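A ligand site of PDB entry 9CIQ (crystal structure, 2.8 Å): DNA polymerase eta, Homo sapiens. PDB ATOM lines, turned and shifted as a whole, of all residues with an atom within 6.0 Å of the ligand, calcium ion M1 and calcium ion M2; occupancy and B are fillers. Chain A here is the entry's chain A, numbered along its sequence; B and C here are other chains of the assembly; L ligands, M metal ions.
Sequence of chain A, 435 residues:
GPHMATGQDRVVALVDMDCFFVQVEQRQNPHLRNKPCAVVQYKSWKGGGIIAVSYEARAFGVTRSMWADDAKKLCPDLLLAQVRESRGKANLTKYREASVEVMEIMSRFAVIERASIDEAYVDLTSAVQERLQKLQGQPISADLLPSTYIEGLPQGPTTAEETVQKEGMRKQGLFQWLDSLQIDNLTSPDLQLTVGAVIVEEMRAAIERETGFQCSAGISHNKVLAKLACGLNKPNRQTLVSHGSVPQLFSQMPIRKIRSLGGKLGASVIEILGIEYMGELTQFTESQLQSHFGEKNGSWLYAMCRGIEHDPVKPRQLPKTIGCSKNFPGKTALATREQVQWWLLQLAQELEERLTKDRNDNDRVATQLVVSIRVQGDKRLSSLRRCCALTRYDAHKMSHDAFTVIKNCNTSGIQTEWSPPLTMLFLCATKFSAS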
ATOM      1  N   ASP A  16      29.455  15.406  33.098  1.00  0.00           N
ATOM      2  CA  ASP A  16      28.654  15.833  31.962  1.00  0.00           C
ATOM      3  C   ASP A  16      27.848  17.035  32.400  1.00  0.00           C
ATOM      4  O   ASP A  16      26.984  16.907  33.276  1.00  0.00           O
ATOM      5  CB  ASP A  16      27.714  14.711  31.492  1.00  0.00           C
ATOM      6  CG  ASP A  16      27.053  14.980  30.152  1.00  0.00           C
ATOM      7  OD1 ASP A  16      26.811  16.154  29.811  1.00  0.00           O
ATOM      8  OD2 ASP A  16      26.761  14.030  29.409  1.00  0.00           O
ATOM      9  N   MET A  17      28.116  18.194  31.797  1.00  0.00           N
ATOM     10  CA  MET A  17      27.307  19.381  32.083  1.00  0.00           C
ATOM     11  C   MET A  17      25.889  19.189  31.541  1.00  0.00           C
ATOM     12  O   MET A  17      25.691  18.730  30.411  1.00  0.00           O
ATOM     13  CB  MET A  17      27.925  20.647  31.470  1.00  0.00           C
ATOM     14  CG  MET A  17      29.384  20.909  31.843  1.00  0.00           C
ATOM     15  SD  MET A  17      29.746  20.806  33.603  1.00  0.00           S
ATOM     16  CE  MET A  17      28.556  21.998  34.193  1.00  0.00           C
ATOM     17  N   ASP A  18      24.909  19.582  32.342  1.00  0.00           N
ATOM     18  CA  ASP A  18      23.524  19.408  31.966  1.00  0.00           C
ATOM     19  C   ASP A  18      23.071  20.526  31.056  1.00  0.00           C
ATOM     20  O   ASP A  18      23.334  21.691  31.343  1.00  0.00           O
ATOM     21  CB  ASP A  18      22.651  19.380  33.224  1.00  0.00           C
ATOM     22  CG  ASP A  18      23.021  18.261  34.132  1.00  0.00           C
ATOM     23  OD1 ASP A  18      23.170  17.114  33.637  1.00  0.00           O
ATOM     24  OD2 ASP A  18      23.214  18.530  35.307  1.00  0.00           O
ATOM     25  N   CYS A  19      22.347  20.154  29.986  1.00  0.00           N
ATOM     26  CA  CYS A  19      21.921  21.070  28.925  1.00  0.00           C
ATOM     27  C   CYS A  19      22.839  22.290  28.854  1.00  0.00           C
ATOM     28  O   CYS A  19      22.468  23.398  29.238  1.00  0.00           O
ATOM     29  CB  CYS A  19      20.445  21.486  29.084  1.00  0.00           C
ATOM     30  SG  CYS A  19      19.886  22.071  30.696  1.00  0.00           S
ATOM     31  N   PHE A  20      24.053  22.070  28.366  1.00  0.00           N
ATOM     32  CA  PHE A  20      25.130  22.996  28.632  1.00  0.00           C
ATOM     33  C   PHE A  20      24.860  24.347  28.013  1.00  0.00           C
ATOM     34  O   PHE A  20      24.854  25.369  28.702  1.00  0.00           O
ATOM     35  CB  PHE A  20      26.427  22.434  28.108  1.00  0.00           C
ATOM     36  CG  PHE A  20      27.588  23.249  28.459  1.00  0.00           C
ATOM     37  CD1 PHE A  20      27.669  23.832  29.700  1.00  0.00           C
ATOM     38  CD2 PHE A  20      28.619  23.433  27.560  1.00  0.00           C
ATOM     39  CE1 PHE A  20      28.756  24.616  30.042  1.00  0.00           C
ATOM     40  CE2 PHE A  20      29.714  24.187  27.896  1.00  0.00           C
ATOM     41  CZ  PHE A  20      29.792  24.779  29.143  1.00  0.00           C
ATOM     42  N   PHE A  21      24.684  24.384  26.687  1.00  0.00           N
ATOM     43  CA  PHE A  21      24.433  25.643  26.010  1.00  0.00           C
ATOM     44  C   PHE A  21      23.258  26.367  26.651  1.00  0.00           C
ATOM     45  O   PHE A  21      23.332  27.579  26.882  1.00  0.00           O
ATOM     46  CB  PHE A  21      24.181  25.435  24.529  1.00  0.00           C
ATOM     47  CG  PHE A  21      25.345  24.836  23.779  1.00  0.00           C
ATOM     48  CD1 PHE A  21      26.567  24.664  24.373  1.00  0.00           C
ATOM     49  CD2 PHE A  21      25.198  24.465  22.457  1.00  0.00           C
ATOM     50  CE1 PHE A  21      27.617  24.122  23.668  1.00  0.00           C
ATOM     51  CE2 PHE A  21      26.251  23.910  21.756  1.00  0.00           C
ATOM     52  CZ  PHE A  21      27.460  23.738  22.362  1.00  0.00           C
ATOM     53  N   VAL A  22      22.199  25.626  26.997  1.00  0.00           N
ATOM     54  CA  VAL A  22      21.054  26.240  27.675  1.00  0.00           C
ATOM     55  C   VAL A  22      21.469  26.830  29.020  1.00  0.00           C
ATOM     56  O   VAL A  22      21.091  27.948  29.363  1.00  0.00           O
ATOM     57  CB  VAL A  22      19.918  25.227  27.849  1.00  0.00           C
ATOM     58  CG1 VAL A  22      18.737  25.896  28.537  1.00  0.00           C
ATOM     59  CG2 VAL A  22      19.515  24.626  26.509  1.00  0.00           C
ATOM     60  N   ILE A  51      19.685  23.018  18.933  1.00  0.00           N
ATOM     61  CA  ILE A  51      20.884  22.303  19.327  1.00  0.00           C
ATOM     62  C   ILE A  51      20.969  22.052  20.812  1.00  0.00           C
ATOM     63  O   ILE A  51      21.900  21.348  21.245  1.00  0.00           O
ATOM     64  CB  ILE A  51      22.159  23.011  18.832  1.00  0.00           C
ATOM     65  CG1 ILE A  51      22.270  24.431  19.396  1.00  0.00           C
ATOM     66  CG2 ILE A  51      22.231  22.963  17.303  1.00  0.00           C
ATOM     67  CD1 ILE A  51      23.578  25.099  19.019  1.00  0.00           C
ATOM     68  N   ALA A  52      20.043  22.574  21.612  1.00  0.00           N
ATOM     69  CA  ALA A  52      19.992  22.235  23.029  1.00  0.00           C
ATOM     70  C   ALA A  52      18.604  22.580  23.522  1.00  0.00           C
ATOM     71  O   ALA A  52      17.915  23.418  22.940  1.00  0.00           O
ATOM     72  CB  ALA A  52      21.043  22.991  23.848  1.00  0.00           C
ATOM     73  N   VAL A  53      18.183  21.883  24.578  1.00  0.00           N
ATOM     74  CA  VAL A  53      16.806  21.959  25.056  1.00  0.00           C
ATOM     75  C   VAL A  53      16.832  21.944  26.582  1.00  0.00           C
ATOM     76  O   VAL A  53      17.309  20.976  27.185  1.00  0.00           O
ATOM     77  CB  VAL A  53      15.936  20.799  24.528  1.00  0.00           C
ATOM     78  CG1 VAL A  53      14.467  21.059  24.801  1.00  0.00           C
ATOM     79  CG2 VAL A  53      16.201  20.543  23.059  1.00  0.00           C
ATOM     80  N   TYR A  55      15.261  21.473  30.305  1.00  0.00           N
ATOM     81  CA  TYR A  55      14.434  20.337  30.737  1.00  0.00           C
ATOM     82  C   TYR A  55      12.954  20.696  30.730  1.00  0.00           C
ATOM     83  O   TYR A  55      12.115  19.853  30.413  1.00  0.00           O
ATOM     84  CB  TYR A  55      14.869  19.845  32.123  1.00  0.00           C
ATOM     85  CG  TYR A  55      16.089  18.921  32.079  1.00  0.00           C
ATOM     86  CD1 TYR A  55      17.341  19.414  31.779  1.00  0.00           C
ATOM     87  CD2 TYR A  55      15.969  17.561  32.356  1.00  0.00           C
ATOM     88  CE1 TYR A  55      18.466  18.592  31.739  1.00  0.00           C
ATOM     89  CE2 TYR A  55      17.092  16.707  32.307  1.00  0.00           C
ATOM     90  CZ  TYR A  55      18.349  17.229  32.002  1.00  0.00           C
ATOM     91  OH  TYR A  55      19.481  16.422  31.960  1.00  0.00           O
ATOM     92  N   ARG A  58      11.965  20.028  27.119  1.00  0.00           N
ATOM     93  CA  ARG A  58      11.935  18.584  26.872  1.00  0.00           C
ATOM     94  C   ARG A  58      10.589  18.003  27.304  1.00  0.00           C
ATOM     95  O   ARG A  58      10.018  17.158  26.600  1.00  0.00           O
ATOM     96  CB  ARG A  58      13.082  17.897  27.626  1.00  0.00           C
ATOM     97  CG  ARG A  58      14.452  18.428  27.246  1.00  0.00           C
ATOM     98  CD  ARG A  58      15.615  17.754  27.948  1.00  0.00           C
ATOM     99  NE  ARG A  58      16.867  18.326  27.463  1.00  0.00           N
ATOM    100  CZ  ARG A  58      18.088  18.063  27.928  1.00  0.00           C
ATOM    101  NH1 ARG A  58      18.291  17.129  28.844  1.00  0.00           N
ATOM    102  NH2 ARG A  58      19.118  18.778  27.470  1.00  0.00           N
ATOM    103  N   ARG A  64      16.798  17.886  20.204  1.00  0.00           N
ATOM    104  CA  ARG A  64      17.912  18.403  19.422  1.00  0.00           C
ATOM    105  C   ARG A  64      17.712  18.101  17.942  1.00  0.00           C
ATOM    106  O   ARG A  64      16.945  17.217  17.553  1.00  0.00           O
ATOM    107  CB  ARG A  64      19.226  17.789  19.928  1.00  0.00           C
ATOM    108  CG  ARG A  64      20.486  18.363  19.326  1.00  0.00           C
ATOM    109  CD  ARG A  64      21.709  17.725  19.922  1.00  0.00           C
ATOM    110  NE  ARG A  64      21.452  16.362  20.349  1.00  0.00           N
ATOM    111  CZ  ARG A  64      21.642  15.906  21.588  1.00  0.00           C
ATOM    112  NH1 ARG A  64      22.129  16.678  22.541  1.00  0.00           N
ATOM    113  NH2 ARG A  64      21.347  14.638  21.862  1.00  0.00           N
ATOM    114  N   SER A  65      18.417  18.872  17.090  1.00  0.00           N
ATOM    115  CA  SER A  65      18.372  18.739  15.635  1.00  0.00           C
ATOM    116  C   SER A  65      16.999  19.109  15.058  1.00  0.00           C
ATOM    117  O   SER A  65      16.894  19.470  13.877  1.00  0.00           O
ATOM    118  CB  SER A  65      18.765  17.326  15.224  1.00  0.00           C
ATOM    119  OG  SER A  65      20.036  16.987  15.738  1.00  0.00           O
ATOM    120  N   SER A 116      34.685  16.096  25.452  1.00  0.00           N
ATOM    121  CA  SER A 116      33.949  16.954  24.540  1.00  0.00           C
ATOM    122  C   SER A 116      33.924  18.351  25.147  1.00  0.00           C
ATOM    123  O   SER A 116      34.556  18.618  26.162  1.00  0.00           O
ATOM    124  CB  SER A 116      32.549  16.382  24.303  1.00  0.00           C
ATOM    125  OG  SER A 116      31.676  16.658  25.387  1.00  0.00           O
ATOM    126  N   ILE A 117      33.161  19.262  24.528  1.00  0.00           N
ATOM    127  CA  ILE A 117      32.979  20.577  25.127  1.00  0.00           C
ATOM    128  C   ILE A 117      32.325  20.462  26.499  1.00  0.00           C
ATOM    129  O   ILE A 117      32.551  21.283  27.396  1.00  0.00           O
ATOM    130  CB  ILE A 117      32.152  21.452  24.178  1.00  0.00           C
ATOM    131  CG1 ILE A 117      32.211  22.901  24.629  1.00  0.00           C
ATOM    132  CG2 ILE A 117      30.714  20.942  24.097  1.00  0.00           C
ATOM    133  CD1 ILE A 117      31.452  23.827  23.771  1.00  0.00           C
ATOM    134  N   ASP A 118      31.582  19.389  26.700  1.00  0.00           N
ATOM    135  CA  ASP A 118      30.614  19.138  27.758  1.00  0.00           C
ATOM    136  C   ASP A 118      31.124  18.137  28.801  1.00  0.00           C
ATOM    137  O   ASP A 118      30.529  18.051  29.885  1.00  0.00           O
ATOM    138  CB  ASP A 118      29.340  18.600  27.060  1.00  0.00           C
ATOM    139  CG  ASP A 118      28.072  18.755  27.861  1.00  0.00           C
ATOM    140  OD1 ASP A 118      28.099  18.570  29.092  1.00  0.00           O
ATOM    141  OD2 ASP A 118      27.002  19.002  27.246  1.00  0.00           O
ATOM    142  N   GLU A 119      32.180  17.374  28.513  1.00  0.00           N
ATOM    143  CA  GLU A 119      32.478  16.191  29.309  1.00  0.00           C
ATOM    144  C   GLU A 119      33.958  16.069  29.643  1.00  0.00           C
ATOM    145  O   GLU A 119      34.818  16.359  28.820  1.00  0.00           O
ATOM    146  CB  GLU A 119      32.051  14.908  28.580  1.00  0.00           C
ATOM    147  CG  GLU A 119      30.595  14.869  28.204  1.00  0.00           C
ATOM    148  CD  GLU A 119      30.175  13.516  27.727  1.00  0.00           C
ATOM    149  OE1 GLU A 119      31.024  12.607  27.722  1.00  0.00           O
ATOM    150  OE2 GLU A 119      28.997  13.344  27.354  1.00  0.00           O
ATOM    151  N   LYS A 234      19.883  12.018  35.894  1.00  0.00           N
ATOM    152  CA  LYS A 234      20.096  13.384  35.480  1.00  0.00           C
ATOM    153  C   LYS A 234      18.835  14.177  35.772  1.00  0.00           C
ATOM    154  O   LYS A 234      17.747  13.597  35.806  1.00  0.00           O
ATOM    155  CB  LYS A 234      20.439  13.485  33.989  1.00  0.00           C
ATOM    156  CG  LYS A 234      21.793  12.923  33.630  1.00  0.00           C
ATOM    157  CD  LYS A 234      22.048  13.090  32.144  1.00  0.00           C
ATOM    158  CE  LYS A 234      23.357  13.794  31.907  1.00  0.00           C
ATOM    159  NZ  LYS A 234      23.518  14.073  30.466  1.00  0.00           N
ATOM    160  P    DT B   8      29.951  10.048  23.653  1.00  0.00           P
ATOM    161  OP1  DT B   8      30.828  10.026  24.845  1.00  0.00           O
ATOM    162  OP2  DT B   8      28.590   9.450  23.673  1.00  0.00           O
ATOM    163  O5'  DT B   8      29.780  11.559  23.160  1.00  0.00           O
ATOM    164  C5'  DT B   8      30.879  12.422  23.245  1.00  0.00           C
ATOM    165  C4'  DT B   8      30.466  13.840  22.914  1.00  0.00           C
ATOM    166  O4'  DT B   8      30.366  13.983  21.478  1.00  0.00           O
ATOM    167  C3'  DT B   8      29.121  14.263  23.480  1.00  0.00           C
ATOM    168  O3'  DT B   8      29.290  15.442  24.224  1.00  0.00           O
ATOM    169  C2'  DT B   8      28.262  14.513  22.244  1.00  0.00           C
ATOM    170  C1'  DT B   8      29.306  14.833  21.195  1.00  0.00           C
ATOM    171  N1   DT B   8      28.856  14.561  19.813  1.00  0.00           N
ATOM    172  C2   DT B   8      29.096  15.498  18.846  1.00  0.00           C
ATOM    173  O2   DT B   8      29.661  16.523  19.061  1.00  0.00           O
ATOM    174  N3   DT B   8      28.624  15.176  17.610  1.00  0.00           N
ATOM    175  C4   DT B   8      27.977  14.018  17.251  1.00  0.00           C
ATOM    176  O4   DT B   8      27.608  13.820  16.106  1.00  0.00           O
ATOM    177  C5   DT B   8      27.767  13.072  18.307  1.00  0.00           C
ATOM    178  C7   DT B   8      27.064  11.794  18.014  1.00  0.00           C
ATOM    179  C6   DT B   8      28.212  13.379  19.534  1.00  0.00           C
ATOM    180  P    DA C   4      23.013  20.149   8.469  1.00  0.00           P
ATOM    181  OP1  DA C   4      21.951  20.754   7.618  1.00  0.00           O
ATOM    182  OP2  DA C   4      24.409  20.133   7.982  1.00  0.00           O
ATOM    183  O5'  DA C   4      23.117  20.876   9.884  1.00  0.00           O
ATOM    184  C5'  DA C   4      23.035  22.299   9.951  1.00  0.00           C
ATOM    185  C4'  DA C   4      24.105  22.864  10.852  1.00  0.00           C
ATOM    186  O4'  DA C   4      24.295  22.009  12.006  1.00  0.00           O
ATOM    187  C3'  DA C   4      25.469  22.953  10.218  1.00  0.00           C
ATOM    188  O3'  DA C   4      26.168  24.034  10.824  1.00  0.00           O
ATOM    189  C2'  DA C   4      26.079  21.603  10.582  1.00  0.00           C
ATOM    190  C1'  DA C   4      25.595  21.448  11.990  1.00  0.00           C
ATOM    191  N9   DA C   4      25.510  20.065  12.478  1.00  0.00           N
ATOM    192  C8   DA C   4      25.087  18.964  11.792  1.00  0.00           C
ATOM    193  N7   DA C   4      25.090  17.860  12.504  1.00  0.00           N
ATOM    194  C5   DA C   4      25.541  18.274  13.739  1.00  0.00           C
ATOM    195  C6   DA C   4      25.776  17.601  14.938  1.00  0.00           C
ATOM    196  N6   DA C   4      25.578  16.290  15.115  1.00  0.00           N
ATOM    197  N1   DA C   4      26.223  18.311  15.969  1.00  0.00           N
ATOM    198  C2   DA C   4      26.422  19.612  15.809  1.00  0.00           C
ATOM    199  N3   DA C   4      26.234  20.349  14.746  1.00  0.00           N
ATOM    200  C4   DA C   4      25.799  19.622  13.728  1.00  0.00           C
ATOM    201  P    DA C   5      27.363  24.802  10.095  1.00  0.00           P
ATOM    202  OP1  DA C   5      28.701  24.222   9.796  1.00  0.00           O
ATOM    203  OP2  DA C   5      27.087  23.828   9.006  1.00  0.00           O
ATOM    204  O5'  DA C   5      28.275  24.873  11.392  1.00  0.00           O
ATOM    205  C5'  DA C   5      28.291  23.777  12.215  1.00  0.00           C
ATOM    206  C4'  DA C   5      29.234  23.945  13.373  1.00  0.00           C
ATOM    207  O4'  DA C   5      29.074  22.773  14.170  1.00  0.00           O
ATOM    208  C3'  DA C   5      30.721  23.991  13.009  1.00  0.00           C
ATOM    209  O3'  DA C   5      31.475  24.693  14.016  1.00  0.00           O
ATOM    210  C2'  DA C   5      31.095  22.518  12.939  1.00  0.00           C
ATOM    211  C1'  DA C   5      30.185  21.911  14.009  1.00  0.00           C
ATOM    212  N9   DA C   5      29.709  20.565  13.688  1.00  0.00           N
ATOM    213  C8   DA C   5      29.172  20.127  12.508  1.00  0.00           C
ATOM    214  N7   DA C   5      28.836  18.852  12.517  1.00  0.00           N
ATOM    215  C5   DA C   5      29.148  18.427  13.790  1.00  0.00           C
ATOM    216  C6   DA C   5      29.038  17.182  14.435  1.00  0.00           C
ATOM    217  N6   DA C   5      28.543  16.101  13.855  1.00  0.00           N
ATOM    218  N1   DA C   5      29.439  17.100  15.712  1.00  0.00           N
ATOM    219  C2   DA C   5      29.930  18.198  16.302  1.00  0.00           C
ATOM    220  N3   DA C   5      30.105  19.418  15.808  1.00  0.00           N
ATOM    221  C4   DA C   5      29.690  19.468  14.534  1.00  0.00           C
HETATM  222  C1  LIG L   1      25.833  19.019  23.130  1.00  0.00           C
HETATM  223  C2  LIG L   1      26.441  18.442  24.193  1.00  0.00           C
HETATM  224  C3  LIG L   1      28.020  18.650  23.872  1.00  0.00           C
HETATM  225  C4  LIG L   1      26.802  18.853  21.940  1.00  0.00           C
HETATM  226  C5  LIG L   1      26.719  18.393  19.736  1.00  0.00           C
HETATM  227  C6  LIG L   1      25.771  16.922  21.232  1.00  0.00           C
HETATM  228  C7  LIG L   1      25.404  16.119  20.155  1.00  0.00           C
HETATM  229  N1  LIG L   1      26.418  18.062  20.953  1.00  0.00           N
HETATM  230  N2  LIG L   1      26.363  17.614  18.686  1.00  0.00           N
HETATM  231  O1  LIG L   1      25.823  20.442  23.469  1.00  0.00           O
HETATM  232  C8  LIG L   1      24.639  14.792  20.397  1.00  0.00           C
HETATM  233  C9  LIG L   1      25.711  16.487  18.843  1.00  0.00           C
HETATM  234  O2  LIG L   1      22.061  19.406  25.967  1.00  0.00           O
HETATM  235  O3  LIG L   1      24.213  15.386  24.415  1.00  0.00           O
HETATM  236  O4  LIG L   1      28.146  18.326  22.596  1.00  0.00           O
HETATM  237  O5  LIG L   1      27.323  19.407  19.519  1.00  0.00           O
HETATM  238  O6  LIG L   1      25.400  15.791  17.917  1.00  0.00           O
HETATM  239  O7  LIG L   1      26.170  17.046  24.292  1.00  0.00           O
HETATM  240  O8  LIG L   1      25.204  16.253  26.591  1.00  0.00           O
HETATM  241  O9  LIG L   1      23.855  17.815  25.134  1.00  0.00           O
HETATM  242  O10 LIG L   1      24.058  18.965  27.430  1.00  0.00           O
HETATM  243  O11 LIG L   1      22.191  17.133  27.092  1.00  0.00           O
HETATM  244  O12 LIG L   1      23.542  16.873  29.321  1.00  0.00           O
HETATM  245  O13 LIG L   1      21.066  17.212  29.418  1.00  0.00           O
HETATM  246  O14 LIG L   1      21.996  15.121  28.530  1.00  0.00           O
HETATM  247  P1  LIG L   1      24.882  16.554  25.158  1.00  0.00           P
HETATM  248  P2  LIG L   1      23.062  18.391  26.465  1.00  0.00           P
HETATM  249  P3  LIG L   1      22.206  16.596  28.645  1.00  0.00           P
HETATM  250 CA    CA M   1      25.410  17.634  28.537  1.00  0.00          CA
HETATM  251 CA    CA M   2      28.237  15.935  26.551  1.00  0.00          CA
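Merely in contact with the ligand: Ile 117 (3.5 Å), Asp 18 (3.7 Å) and Phe 21 (3.8 Å). 14 residues have an atom within 4 Å of the ligand: Asp 16, Met 17, Asp 18, Cys 19, Phe 20, Phe 21, Tyr 55, Arg 58, Arg 64, Ile 117, Asp 118, Lys 234, DT 8 of chain B and DA 4 of chain C. The nearest printed residue that does not touch the ligand is Ala 52 (4.3 Å).
Of the 22 residues printed, 3 come within 4 Å of calcium ion M1. The nearest printed residue that does not touch calcium ion M1 is Cys 19 (4.2 Å).
NH1 of Arg 64 is in salt-bridge range of O3 of the ligand. The guanidinium group (NH1) of Arg 58 is in salt-bridge range of an oxygen (O13) of the ligand, 2.8 Å away. O13 of the ligand is in hydrogen-bond range of OH of Tyr 55, at 3.1 Å. The backbone NH (N) of Phe 20 lies close to an oxygen (O10) of the ligand, 3.2 Å away. N1 of DA 4 of chain C lies within hydrogen-bond range of N2 of the ligand, at 2.8 Å. The side-chain amino group of Lys 234 lies within salt-bridge range of an oxygen (O14) of the ligand, 2.7 Å away. O2 of DT 8 of chain B lies close to a nitrogen (N2) of the ligand (3.5 Å). The backbone NH (N) of Cys 19 is in hydrogen-bond range of an oxygen (O13) of the ligand, at 3.3 Å.
Calcium ion M2 is bound by O3' of DT 8 of chain B (2.6 Å) and OE2 of Glu 119 (2.8 Å). Slightly farther from calcium ion M2 lies O8 of the ligand (3.0 Å).
OG of Ser 116 touches calcium ion M2 (3.7 Å). Within 4 Å of calcium ion M2: Asp 16, Ser 116, Asp 118, Glu 119 and DT 8 of chain B.
O3' of DT 8 of chain B lies close to the side-chain hydroxyl (OG) of Ser 116, 2.9 Å away. The backbone NH of Asp 118 lies close to the side-chain hydroxyl of Ser 116 (3.0 Å). The side-chain amino group of Lys 234 is in salt-bridge range of the side-chain carboxylate of Asp 16 (3.4 Å). The side-chain hydroxyl of Ser 116 lies within hydrogen-bond range of the backbone NH of Glu 119 (3.2 Å). The guanidinium group (NH1) of Arg 58 sits close to the side-chain hydroxyl (OH) of Tyr 55 (3.4 Å). NE of Arg 58 is in hydrogen-bond range of O of Val 53, 2.7 Å away.
O12 of the ligand binds calcium ion M1. O of Met 17 binds calcium ion M1 (2.2 Å). Calcium ion M1 is bound by an oxygen (O10) of the ligand (2.2 Å). An oxygen (O8) of the ligand binds calcium ion M1. Calcium ion M1 is bound by OD1 of Asp 16 (2.4 Å). Calcium ion M1 is bound by OD2 of Asp 118, at 2.5 Å. Slightly farther from calcium ion M1 lies the side-chain carboxylate (OD1) of Asp 118 (2.9 Å).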
